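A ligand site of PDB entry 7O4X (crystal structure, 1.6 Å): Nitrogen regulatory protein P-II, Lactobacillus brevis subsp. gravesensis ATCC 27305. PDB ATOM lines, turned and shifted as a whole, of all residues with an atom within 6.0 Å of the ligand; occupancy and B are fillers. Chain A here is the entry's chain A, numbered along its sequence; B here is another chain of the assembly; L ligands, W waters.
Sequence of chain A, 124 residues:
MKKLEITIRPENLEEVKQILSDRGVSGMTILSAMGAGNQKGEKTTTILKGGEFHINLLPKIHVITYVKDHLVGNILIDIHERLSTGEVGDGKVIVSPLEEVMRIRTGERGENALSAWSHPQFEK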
ATOM      1  N   VAL A  25      18.473  31.118  19.290  1.00  0.00           N
ATOM      2  CA  VAL A  25      18.814  29.793  18.688  1.00  0.00           C
ATOM      3  C   VAL A  25      20.055  29.198  19.373  1.00  0.00           C
ATOM      4  O   VAL A  25      21.027  29.871  19.490  1.00  0.00           O
ATOM      5  CB  VAL A  25      18.899  29.854  17.173  1.00  0.00           C
ATOM      6  CG1 VAL A  25      19.472  28.597  16.578  1.00  0.00           C
ATOM      7  CG2 VAL A  25      17.526  30.045  16.582  1.00  0.00           C
ATOM      8  N   SER A  26      20.036  27.877  19.673  1.00  0.00           N
ATOM      9  CA  SER A  26      20.958  27.220  20.632  1.00  0.00           C
ATOM     10  C   SER A  26      22.346  26.940  20.001  1.00  0.00           C
ATOM     11  O   SER A  26      23.325  26.877  20.833  1.00  0.00           O
ATOM     12  CB  SER A  26      20.372  25.973  21.231  1.00  0.00           C
ATOM     13  OG  SER A  26      19.964  25.066  20.239  1.00  0.00           O
ATOM     14  N   GLY A  27      22.429  26.911  18.667  1.00  0.00           N
ATOM     15  CA  GLY A  27      23.555  26.317  17.950  1.00  0.00           C
ATOM     16  C   GLY A  27      23.465  26.279  16.443  1.00  0.00           C
ATOM     17  O   GLY A  27      22.421  26.622  15.831  1.00  0.00           O
ATOM     18  N   MET A  28      24.560  25.816  15.816  1.00  0.00           N
ATOM     19  CA  MET A  28      24.705  25.831  14.353  1.00  0.00           C
ATOM     20  C   MET A  28      25.916  24.955  13.990  1.00  0.00           C
ATOM     21  O   MET A  28      26.816  24.825  14.844  1.00  0.00           O
ATOM     22  CB  MET A  28      24.931  27.288  13.896  1.00  0.00           C
ATOM     23  CG  MET A  28      26.082  27.919  14.588  1.00  0.00           C
ATOM     24  SD  MET A  28      26.175  29.711  14.400  1.00  0.00           S
ATOM     25  CE  MET A  28      26.751  29.673  12.714  1.00  0.00           C
ATOM     26  N   THR A  29      25.876  24.363  12.791  1.00  0.00           N
ATOM     27  CA  THR A  29      27.001  23.559  12.227  1.00  0.00           C
ATOM     28  C   THR A  29      27.412  24.220  10.900  1.00  0.00           C
ATOM     29  O   THR A  29      26.512  24.465  10.061  1.00  0.00           O
ATOM     30  CB  THR A  29      26.579  22.117  12.089  1.00  0.00           C
ATOM     31  OG1 THR A  29      26.284  21.602  13.401  1.00  0.00           O
ATOM     32  CG2 THR A  29      27.699  21.275  11.509  1.00  0.00           C
ATOM     33  N   ILE A  64      24.001  25.062   8.729  1.00  0.00           N
ATOM     34  CA  ILE A  64      22.812  24.223   9.095  1.00  0.00           C
ATOM     35  C   ILE A  64      22.439  24.584  10.517  1.00  0.00           C
ATOM     36  O   ILE A  64      23.274  24.658  11.408  1.00  0.00           O
ATOM     37  CB  ILE A  64      23.180  22.734   8.986  1.00  0.00           C
ATOM     38  CG1 ILE A  64      23.511  22.381   7.528  1.00  0.00           C
ATOM     39  CG2 ILE A  64      22.072  21.862   9.560  1.00  0.00           C
ATOM     40  CD1 ILE A  64      24.369  21.122   7.559  1.00  0.00           C
ATOM     41  N   THR A  65      21.141  24.835  10.737  1.00  0.00           N
ATOM     42  CA  THR A  65      20.637  25.066  12.106  1.00  0.00           C
ATOM     43  C   THR A  65      19.235  24.440  12.199  1.00  0.00           C
ATOM     44  O   THR A  65      18.480  24.421  11.237  1.00  0.00           O
ATOM     45  CB  THR A  65      20.696  26.578  12.479  1.00  0.00           C
ATOM     46  OG1 THR A  65      20.336  26.737  13.838  1.00  0.00           O
ATOM     47  CG2 THR A  65      19.801  27.440  11.613  1.00  0.00           C
ATOM     48  N   TYR A  66      18.977  23.875  13.389  1.00  0.00           N
ATOM     49  CA  TYR A  66      17.657  23.268  13.700  1.00  0.00           C
ATOM     50  C   TYR A  66      16.952  24.263  14.622  1.00  0.00           C
ATOM     51  O   TYR A  66      17.586  24.682  15.608  1.00  0.00           O
ATOM     52  CB  TYR A  66      17.838  21.873  14.299  1.00  0.00           C
ATOM     53  CG  TYR A  66      18.768  20.999  13.516  1.00  0.00           C
ATOM     54  CD1 TYR A  66      18.499  20.664  12.195  1.00  0.00           C
ATOM     55  CD2 TYR A  66      19.938  20.511  14.078  1.00  0.00           C
ATOM     56  CE1 TYR A  66      19.356  19.863  11.470  1.00  0.00           C
ATOM     57  CE2 TYR A  66      20.805  19.711  13.353  1.00  0.00           C
ATOM     58  CZ  TYR A  66      20.516  19.378  12.046  1.00  0.00           C
ATOM     59  OH  TYR A  66      21.370  18.595  11.329  1.00  0.00           O
ATOM     60  N   VAL A  67      15.707  24.623  14.328  1.00  0.00           N
ATOM     61  CA  VAL A  67      14.962  25.711  15.020  1.00  0.00           C
ATOM     62  C   VAL A  67      13.499  25.334  15.255  1.00  0.00           C
ATOM     63  O   VAL A  67      12.906  24.520  14.513  1.00  0.00           O
ATOM     64  CB  VAL A  67      15.063  27.046  14.284  1.00  0.00           C
ATOM     65  CG1 VAL A  67      16.497  27.460  13.926  1.00  0.00           C
ATOM     66  CG2 VAL A  67      14.202  27.086  13.041  1.00  0.00           C
ATOM     67  N   ARG A 103      19.231  14.833  21.420  1.00  0.00           N
ATOM     68  CA  ARG A 103      20.519  15.200  22.088  1.00  0.00           C
ATOM     69  C   ARG A 103      21.291  13.951  22.499  1.00  0.00           C
ATOM     70  O   ARG A 103      20.820  13.175  23.327  1.00  0.00           O
ATOM     71  CB  ARG A 103      20.230  16.110  23.317  1.00  0.00           C
ATOM     72  CG  ARG A 103      21.470  16.357  24.168  1.00  0.00           C
ATOM     73  CD  ARG A 103      21.184  17.304  25.337  1.00  0.00           C
ATOM     74  NE  ARG A 103      21.270  18.627  24.803  1.00  0.00           N
ATOM     75  CZ  ARG A 103      20.407  19.642  24.954  1.00  0.00           C
ATOM     76  NH1 ARG A 103      20.683  20.806  24.402  1.00  0.00           N
ATOM     77  NH2 ARG A 103      19.291  19.472  25.635  1.00  0.00           N
ATOM     78  N   ILE A 104      22.514  13.809  21.995  1.00  0.00           N
ATOM     79  CA  ILE A 104      23.332  12.580  22.302  1.00  0.00           C
ATOM     80  C   ILE A 104      23.593  12.451  23.801  1.00  0.00           C
ATOM     81  O   ILE A 104      23.578  11.361  24.359  1.00  0.00           O
ATOM     82  CB  ILE A 104      24.599  12.558  21.408  1.00  0.00           C
ATOM     83  CG1 ILE A 104      24.204  12.468  19.928  1.00  0.00           C
ATOM     84  CG2 ILE A 104      25.539  11.459  21.867  1.00  0.00           C
ATOM     85  CD1 ILE A 104      25.363  12.478  18.971  1.00  0.00           C
ATOM     86  N   ARG A 105      23.973  13.547  24.472  1.00  0.00           N
ATOM     87  CA  ARG A 105      24.407  13.467  25.900  1.00  0.00           C
ATOM     88  C   ARG A 105      23.310  12.915  26.811  1.00  0.00           C
ATOM     89  O   ARG A 105      23.638  12.105  27.695  1.00  0.00           O
ATOM     90  CB  ARG A 105      24.768  14.884  26.380  1.00  0.00           C
ATOM     91  CG  ARG A 105      25.722  14.943  27.558  1.00  0.00           C
ATOM     92  CD  ARG A 105      25.818  16.373  28.035  1.00  0.00           C
ATOM     93  NE  ARG A 105      24.634  17.135  27.675  1.00  0.00           N
ATOM     94  CZ  ARG A 105      24.194  18.214  28.325  1.00  0.00           C
ATOM     95  NH1 ARG A 105      24.857  18.651  29.382  1.00  0.00           N
ATOM     96  NH2 ARG A 105      23.105  18.835  27.920  1.00  0.00           N
ATOM     97  N   ALA A 113      15.488  18.612  23.096  1.00  0.00           N
ATOM     98  CA  ALA A 113      16.838  18.268  22.572  1.00  0.00           C
ATOM     99  C   ALA A 113      17.630  19.512  22.138  1.00  0.00           C
ATOM    100  O   ALA A 113      18.869  19.370  21.870  1.00  0.00           O
ATOM    101  CB  ALA A 113      16.668  17.325  21.423  1.00  0.00           C
ATOM    102  N   LEU A 114      16.974  20.646  21.961  1.00  0.00           N
ATOM    103  CA  LEU A 114      17.608  21.921  21.522  1.00  0.00           C
ATOM    104  C   LEU A 114      17.722  22.960  22.682  1.00  0.00           C
ATOM    105  O   LEU A 114      18.128  24.103  22.382  1.00  0.00           O
ATOM    106  CB  LEU A 114      16.781  22.481  20.361  1.00  0.00           C
ATOM    107  CG  LEU A 114      16.726  21.561  19.125  1.00  0.00           C
ATOM    108  CD1 LEU A 114      15.881  22.168  18.030  1.00  0.00           C
ATOM    109  CD2 LEU A 114      18.121  21.196  18.643  1.00  0.00           C
ATOM    110  N   SER A 115      17.432  22.592  23.935  1.00  0.00           N
ATOM    111  CA  SER A 115      17.452  23.529  25.094  1.00  0.00           C
ATOM    112  C   SER A 115      18.846  24.171  25.291  1.00  0.00           C
ATOM    113  O   SER A 115      19.865  23.583  24.901  1.00  0.00           O
ATOM    114  CB  SER A 115      16.981  22.858  26.368  1.00  0.00           C
ATOM    115  OG  SER A 115      17.904  21.843  26.755  1.00  0.00           O
ATOM    116  N   TRP A 117      21.669  24.824  27.831  1.00  0.00           N
ATOM    117  CA  TRP A 117      22.118  24.112  29.071  1.00  0.00           C
ATOM    118  C   TRP A 117      23.640  23.878  29.023  1.00  0.00           C
ATOM    119  O   TRP A 117      24.296  23.893  30.111  1.00  0.00           O
ATOM    120  CB  TRP A 117      21.358  22.781  29.259  1.00  0.00           C
ATOM    121  N   THR B   7      25.865  14.668  14.153  1.00  0.00           N
ATOM    122  CA  THR B   7      26.916  15.709  14.340  1.00  0.00           C
ATOM    123  C   THR B   7      27.644  15.446  15.665  1.00  0.00           C
ATOM    124  O   THR B   7      26.996  15.542  16.730  1.00  0.00           O
ATOM    125  CB  THR B   7      26.344  17.130  14.297  1.00  0.00           C
ATOM    126  OG1 THR B   7      25.581  17.312  13.093  1.00  0.00           O
ATOM    127  CG2 THR B   7      27.480  18.136  14.342  1.00  0.00           C
ATOM    128  N   MET B  34      32.643  22.863  11.619  1.00  0.00           N
ATOM    129  CA  MET B  34      32.868  23.623  12.882  1.00  0.00           C
ATOM    130  C   MET B  34      31.477  23.808  13.528  1.00  0.00           C
ATOM    131  O   MET B  34      30.512  24.030  12.794  1.00  0.00           O
ATOM    132  CB  MET B  34      33.582  24.931  12.677  1.00  0.00           C
ATOM    133  CG  MET B  34      34.945  24.731  12.005  1.00  0.00           C
ATOM    134  SD  MET B  34      36.170  24.162  13.159  1.00  0.00           S
ATOM    135  CE  MET B  34      36.372  25.601  14.065  1.00  0.00           C
ATOM    136  N   GLY B  35      31.384  23.653  14.852  1.00  0.00           N
ATOM    137  CA  GLY B  35      30.051  23.791  15.474  1.00  0.00           C
ATOM    138  C   GLY B  35      30.096  24.759  16.622  1.00  0.00           C
ATOM    139  O   GLY B  35      31.148  25.019  17.266  1.00  0.00           O
ATOM    140  N   ALA B  36      28.938  25.380  16.907  1.00  0.00           N
ATOM    141  CA  ALA B  36      28.716  26.247  18.080  1.00  0.00           C
ATOM    142  C   ALA B  36      27.437  25.792  18.799  1.00  0.00           C
ATOM    143  O   ALA B  36      26.510  25.275  18.134  1.00  0.00           O
ATOM    144  CB  ALA B  36      28.544  27.670  17.676  1.00  0.00           C
ATOM    145  N   GLY B  37      27.437  25.920  20.112  1.00  0.00           N
ATOM    146  CA  GLY B  37      26.237  25.543  20.910  1.00  0.00           C
ATOM    147  C   GLY B  37      26.484  25.905  22.364  1.00  0.00           C
ATOM    148  O   GLY B  37      27.153  26.931  22.644  1.00  0.00           O
ATOM    149  N   ASN B  38      26.098  24.999  23.272  1.00  0.00           N
ATOM    150  CA  ASN B  38      26.252  25.138  24.750  1.00  0.00           C
ATOM    151  C   ASN B  38      27.722  25.015  25.219  1.00  0.00           C
ATOM    152  O   ASN B  38      28.101  25.627  26.244  1.00  0.00           O
ATOM    153  CB  ASN B  38      25.360  24.078  25.410  1.00  0.00           C
ATOM    154  CG  ASN B  38      23.880  24.343  25.196  1.00  0.00           C
ATOM    155  OD1 ASN B  38      23.441  25.487  25.363  1.00  0.00           O
ATOM    156  ND2 ASN B  38      23.118  23.317  24.881  1.00  0.00           N
ATOM    157  N   GLN B  39      28.542  24.150  24.602  1.00  0.00           N
ATOM    158  CA  GLN B  39      29.932  23.910  25.107  1.00  0.00           C
ATOM    159  C   GLN B  39      30.748  25.235  25.106  1.00  0.00           C
ATOM    160  O   GLN B  39      30.766  25.905  24.068  1.00  0.00           O
ATOM    161  CB  GLN B  39      30.587  22.803  24.273  1.00  0.00           C
ATOM    162  CG  GLN B  39      32.047  22.615  24.684  1.00  0.00           C
ATOM    163  CD  GLN B  39      32.686  21.293  24.317  1.00  0.00           C
ATOM    164  OE1 GLN B  39      32.215  20.530  23.477  1.00  0.00           O
ATOM    165  NE2 GLN B  39      33.825  21.054  24.953  1.00  0.00           N
ATOM    166  N   LEU B  58      34.055  24.966  17.539  1.00  0.00           N
ATOM    167  CA  LEU B  58      34.840  23.749  17.854  1.00  0.00           C
ATOM    168  C   LEU B  58      34.755  22.831  16.655  1.00  0.00           C
ATOM    169  O   LEU B  58      33.722  22.637  16.014  1.00  0.00           O
ATOM    170  CB  LEU B  58      34.299  23.070  19.120  1.00  0.00           C
ATOM    171  CG  LEU B  58      34.462  23.899  20.406  1.00  0.00           C
ATOM    172  CD1 LEU B  58      33.596  23.380  21.506  1.00  0.00           C
ATOM    173  CD2 LEU B  58      35.878  23.913  20.894  1.00  0.00           C
ATOM    174  N   LYS B  60      34.034  19.573  14.452  1.00  0.00           N
ATOM    175  CA  LYS B  60      33.010  18.512  14.451  1.00  0.00           C
ATOM    176  C   LYS B  60      33.136  17.658  13.183  1.00  0.00           C
ATOM    177  O   LYS B  60      33.813  18.046  12.208  1.00  0.00           O
ATOM    178  CB  LYS B  60      31.588  19.053  14.563  1.00  0.00           C
ATOM    179  CG  LYS B  60      31.282  19.938  15.741  1.00  0.00           C
ATOM    180  CD  LYS B  60      31.306  19.170  17.049  1.00  0.00           C
ATOM    181  CE  LYS B  60      31.203  20.056  18.252  1.00  0.00           C
ATOM    182  NZ  LYS B  60      31.415  19.307  19.487  1.00  0.00           N
ATOM    183  N   GLU B  87      29.121  15.011  29.326  1.00  0.00           N
ATOM    184  CA  GLU B  87      29.739  16.357  29.276  1.00  0.00           C
ATOM    185  C   GLU B  87      29.061  17.113  28.129  1.00  0.00           C
ATOM    186  O   GLU B  87      28.801  16.512  27.045  1.00  0.00           O
ATOM    187  CB  GLU B  87      31.261  16.338  29.013  1.00  0.00           C
ATOM    188  CG  GLU B  87      32.075  15.676  30.121  1.00  0.00           C
ATOM    189  CD  GLU B  87      32.024  16.336  31.487  1.00  0.00           C
ATOM    190  OE1 GLU B  87      31.587  17.521  31.583  1.00  0.00           O
ATOM    191  OE2 GLU B  87      32.459  15.682  32.458  1.00  0.00           O
ATOM    192  N   VAL B  88      28.801  18.398  28.317  1.00  0.00           N
ATOM    193  CA  VAL B  88      28.174  19.212  27.234  1.00  0.00           C
ATOM    194  C   VAL B  88      29.053  19.171  25.954  1.00  0.00           C
ATOM    195  O   VAL B  88      30.275  19.272  26.061  1.00  0.00           O
ATOM    196  CB  VAL B  88      27.924  20.647  27.744  1.00  0.00           C
ATOM    197  CG1 VAL B  88      27.440  21.571  26.638  1.00  0.00           C
ATOM    198  CG2 VAL B  88      26.973  20.629  28.929  1.00  0.00           C
ATOM    199  N   GLY B  89      28.414  18.991  24.795  1.00  0.00           N
ATOM    200  CA  GLY B  89      29.061  18.993  23.478  1.00  0.00           C
ATOM    201  C   GLY B  89      29.010  17.639  22.767  1.00  0.00           C
ATOM    202  O   GLY B  89      29.640  17.526  21.686  1.00  0.00           O
ATOM    203  N   ASP B  90      28.342  16.629  23.320  1.00  0.00           N
ATOM    204  CA  ASP B  90      28.354  15.267  22.677  1.00  0.00           C
ATOM    205  C   ASP B  90      27.735  15.301  21.258  1.00  0.00           C
ATOM    206  O   ASP B  90      28.163  14.447  20.441  1.00  0.00           O
ATOM    207  CB  ASP B  90      27.702  14.193  23.539  1.00  0.00           C
ATOM    208  CG  ASP B  90      28.446  13.830  24.799  1.00  0.00           C
ATOM    209  OD1 ASP B  90      29.637  14.050  24.849  1.00  0.00           O
ATOM    210  OD2 ASP B  90      27.785  13.345  25.721  1.00  0.00           O
ATOM    211  N   GLY B  91      26.758  16.164  20.976  1.00  0.00           N
ATOM    212  CA  GLY B  91      26.227  16.400  19.633  1.00  0.00           C
ATOM    213  C   GLY B  91      24.717  16.079  19.514  1.00  0.00           C
ATOM    214  O   GLY B  91      23.994  15.957  20.517  1.00  0.00           O
ATOM    215  N   LYS B  92      24.302  15.893  18.278  1.00  0.00           N
ATOM    216  CA  LYS B  92      22.865  15.831  17.892  1.00  0.00           C
ATOM    217  C   LYS B  92      22.673  14.727  16.853  1.00  0.00           C
ATOM    218  O   LYS B  92      23.605  14.482  16.016  1.00  0.00           O
ATOM    219  CB  LYS B  92      22.393  17.141  17.251  1.00  0.00           C
ATOM    220  CG  LYS B  92      22.568  18.384  18.089  1.00  0.00           C
ATOM    221  CD  LYS B  92      21.856  18.461  19.401  1.00  0.00           C
ATOM    222  CE  LYS B  92      21.994  19.889  19.949  1.00  0.00           C
ATOM    223  NZ  LYS B  92      21.822  19.970  21.411  1.00  0.00           N
HETATM  224  P1  LIG L   1      24.782  19.599  23.926  1.00  0.00           P
HETATM  225  O1  LIG L   1      23.922  19.122  22.860  1.00  0.00           O
HETATM  226  O2  LIG L   1      24.126  20.662  24.861  1.00  0.00           O
HETATM  227  O3  LIG L   1      25.573  18.507  24.695  1.00  0.00           O
HETATM  228  P2  LIG L   1      26.167  21.629  22.224  1.00  0.00           P
HETATM  229  O4  LIG L   1      25.010  22.590  22.487  1.00  0.00           O
HETATM  230  O5  LIG L   1      27.512  22.218  22.577  1.00  0.00           O
HETATM  231  O6  LIG L   1      26.030  20.279  23.109  1.00  0.00           O
HETATM  232  O7  LIG L   1      26.110  21.048  20.738  1.00  0.00           O
HETATM  233  C1  LIG L   1      27.180  20.324  20.146  1.00  0.00           C
HETATM  234  C2  LIG L   1      27.206  20.493  18.638  1.00  0.00           C
HETATM  235  O8  LIG L   1      25.937  20.136  18.005  1.00  0.00           O
HETATM  236  C3  LIG L   1      27.466  21.934  18.203  1.00  0.00           C
HETATM  237  O9  LIG L   1      28.854  22.250  18.287  1.00  0.00           O
HETATM  238  C4  LIG L   1      26.879  21.962  16.811  1.00  0.00           C
HETATM  239  O10 LIG L   1      27.718  21.362  15.868  1.00  0.00           O
HETATM  240  C5  LIG L   1      25.635  21.078  16.979  1.00  0.00           C
HETATM  241  N1  LIG L   1      24.422  21.845  17.340  1.00  0.00           N
HETATM  242  C6  LIG L   1      24.000  22.295  18.586  1.00  0.00           C
HETATM  243  N2  LIG L   1      22.859  22.953  18.538  1.00  0.00           N
HETATM  244  C7  LIG L   1      22.483  22.938  17.174  1.00  0.00           C
HETATM  245  C8  LIG L   1      21.402  23.486  16.455  1.00  0.00           C
HETATM  246  N3  LIG L   1      20.363  24.145  17.006  1.00  0.00           N
HETATM  247  N4  LIG L   1      21.387  23.263  15.125  1.00  0.00           N
HETATM  248  C9  LIG L   1      22.404  22.607  14.534  1.00  0.00           C
HETATM  249  N5  LIG L   1      23.482  22.067  15.104  1.00  0.00           N
HETATM  250  C10 LIG L   1      23.435  22.234  16.438  1.00  0.00           C
HETATM  251  O   HOH W   1      22.298  22.824  21.794  1.00  0.00           O
HETATM  252  O   HOH W   2      29.389  23.152  20.722  1.00  0.00           O
HETATM  253  O   HOH W   3      24.737  16.108  23.295  1.00  0.00           O
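The side-chain amino group of Lys 92 of chain B lies within salt-bridge range of an oxygen (O1) of the ligand. The backbone NH (N) of Asn 38 of chain B is in hydrogen-bond range of an oxygen (O4) of the ligand (2.8 Å). ND2 of Asn 38 of chain B is in hydrogen-bond range of O2 of the ligand, 2.8 Å away. O10 of the ligand is in hydrogen-bond range of OG1 of Thr 29 (2.9 Å). An oxygen (O3) of the ligand sits at hydrogen-bond distance from the backbone NH (N) of Gly 89 of chain B (2.9 Å). N of Gln 39 of chain B lies within hydrogen-bond range of O5 of the ligand (3.0 Å). The backbone NH (N) of Tyr 66 sits at hydrogen-bond distance from a nitrogen (N4) of the ligand, 3.0 Å away. O of Tyr 66 is in hydrogen-bond range of N3 of the ligand (3.2 Å). The guanidinium group (NE) of Arg 103 lies within salt-bridge range of an oxygen (O1) of the ligand (3.3 Å). The backbone carbonyl oxygen (O) of Gly 27 sits close to a nitrogen (N3) of the ligand, 3.4 Å away. N3 of the ligand lies within hydrogen-bond range of OG of Ser 26 (3.4 Å). O3 of the ligand lies within salt-bridge range of NE of Arg 105 (3.4 Å). An oxygen (O9) of the ligand is in hydrogen-bond range of the backbone NH (N) of Ala 36 of chain B (3.4 Å).
The backbone carbonyl oxygen (O) of Ala 113 is in hydrogen-bond range of the side-chain amino group (NZ) of Lys 92 of chain B (3.0 Å). ND2 of Asn 38 of chain B lies within hydrogen-bond range of O of Ser 115. The side-chain amide oxygen (OD1) of Asn 38 of chain B lies within hydrogen-bond range of the backbone NH (N) of Trp 117, 3.1 Å away. O of Val 88 of chain B sits close to OE1 of Gln 39 of chain B. The backbone NH of Gly 35 of chain B is in hydrogen-bond range of the backbone carbonyl oxygen of Leu 58 of chain B. The guanidinium group (NH1) of Arg 103 is in hydrogen-bond range of the backbone carbonyl oxygen (O) of Ala 113 (3.4 Å). O of Gly 27 lies within hydrogen-bond range of OG1 of Thr 65, 2.9 Å away. The side-chain hydroxyl of Ser 26 is in hydrogen-bond range of the backbone carbonyl oxygen of Leu 114, at 3.0 Å.
O of Met 28 touches C4 of the ligand, at 3.5 Å. Ile 64 touches the ligand (O to C9, 3.8 Å). CA of Thr 65 touches N4 of the ligand, at 3.6 Å. Thr 7 of chain B touches the ligand. Gly 35 of chain B touches the ligand. Gly 37 of chain B touches the ligand. Lys 60 of chain B touches the ligand (CE to O9, 3.2 Å). CA of Val 88 of chain B touches O3 of the ligand, 3.7 Å away. Asp 90 of chain B touches the ligand. O of Gly 91 of chain B touches O1 of the ligand, at 3.9 Å. Hydrophobic or aromatic side chains that line the ligand: Tyr 66 and Val 88 of chain B. Within 4 Å of the ligand: Ser 26, Gly 27, Met 28, Thr 29, Ile 64, Thr 65, Tyr 66, Arg 103, Arg 105, Thr 7 of chain B, Gly 35 of chain B, Ala 36 of chain B, Gly 37 of chain B, Asn 38 of chain B, Gln 39 of chain B, Lys 60 of chain B, Val 88 of chain B, Gly 89 of chain B, Asp 90 of chain B, Gly 91 of chain B and Lys 92 of chain B. The nearest printed residue that does not touch the ligand is Leu 114 (4.1 Å).
Water W2 lies within hydrogen-bond range of an oxygen (O9) of the ligand (2.7 Å) and the backbone NH of Gly 37 of chain B (3.4 Å). Water W1 lies within hydrogen-bond range of an oxygen (O4) of the ligand (2.8 Å), the side-chain amino group (NZ) of Lys 92 of chain B (2.9 Å) and the side-chain amide nitrogen (ND2) of Asn 38 of chain B (3.2 Å). Water W3 lies within hydrogen-bond range of O of Gly 91 of chain B (2.9 Å), O3 of the ligand (2.9 Å), N of Arg 105 (2.9 Å) and N of Ile 104 (3.5 Å).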
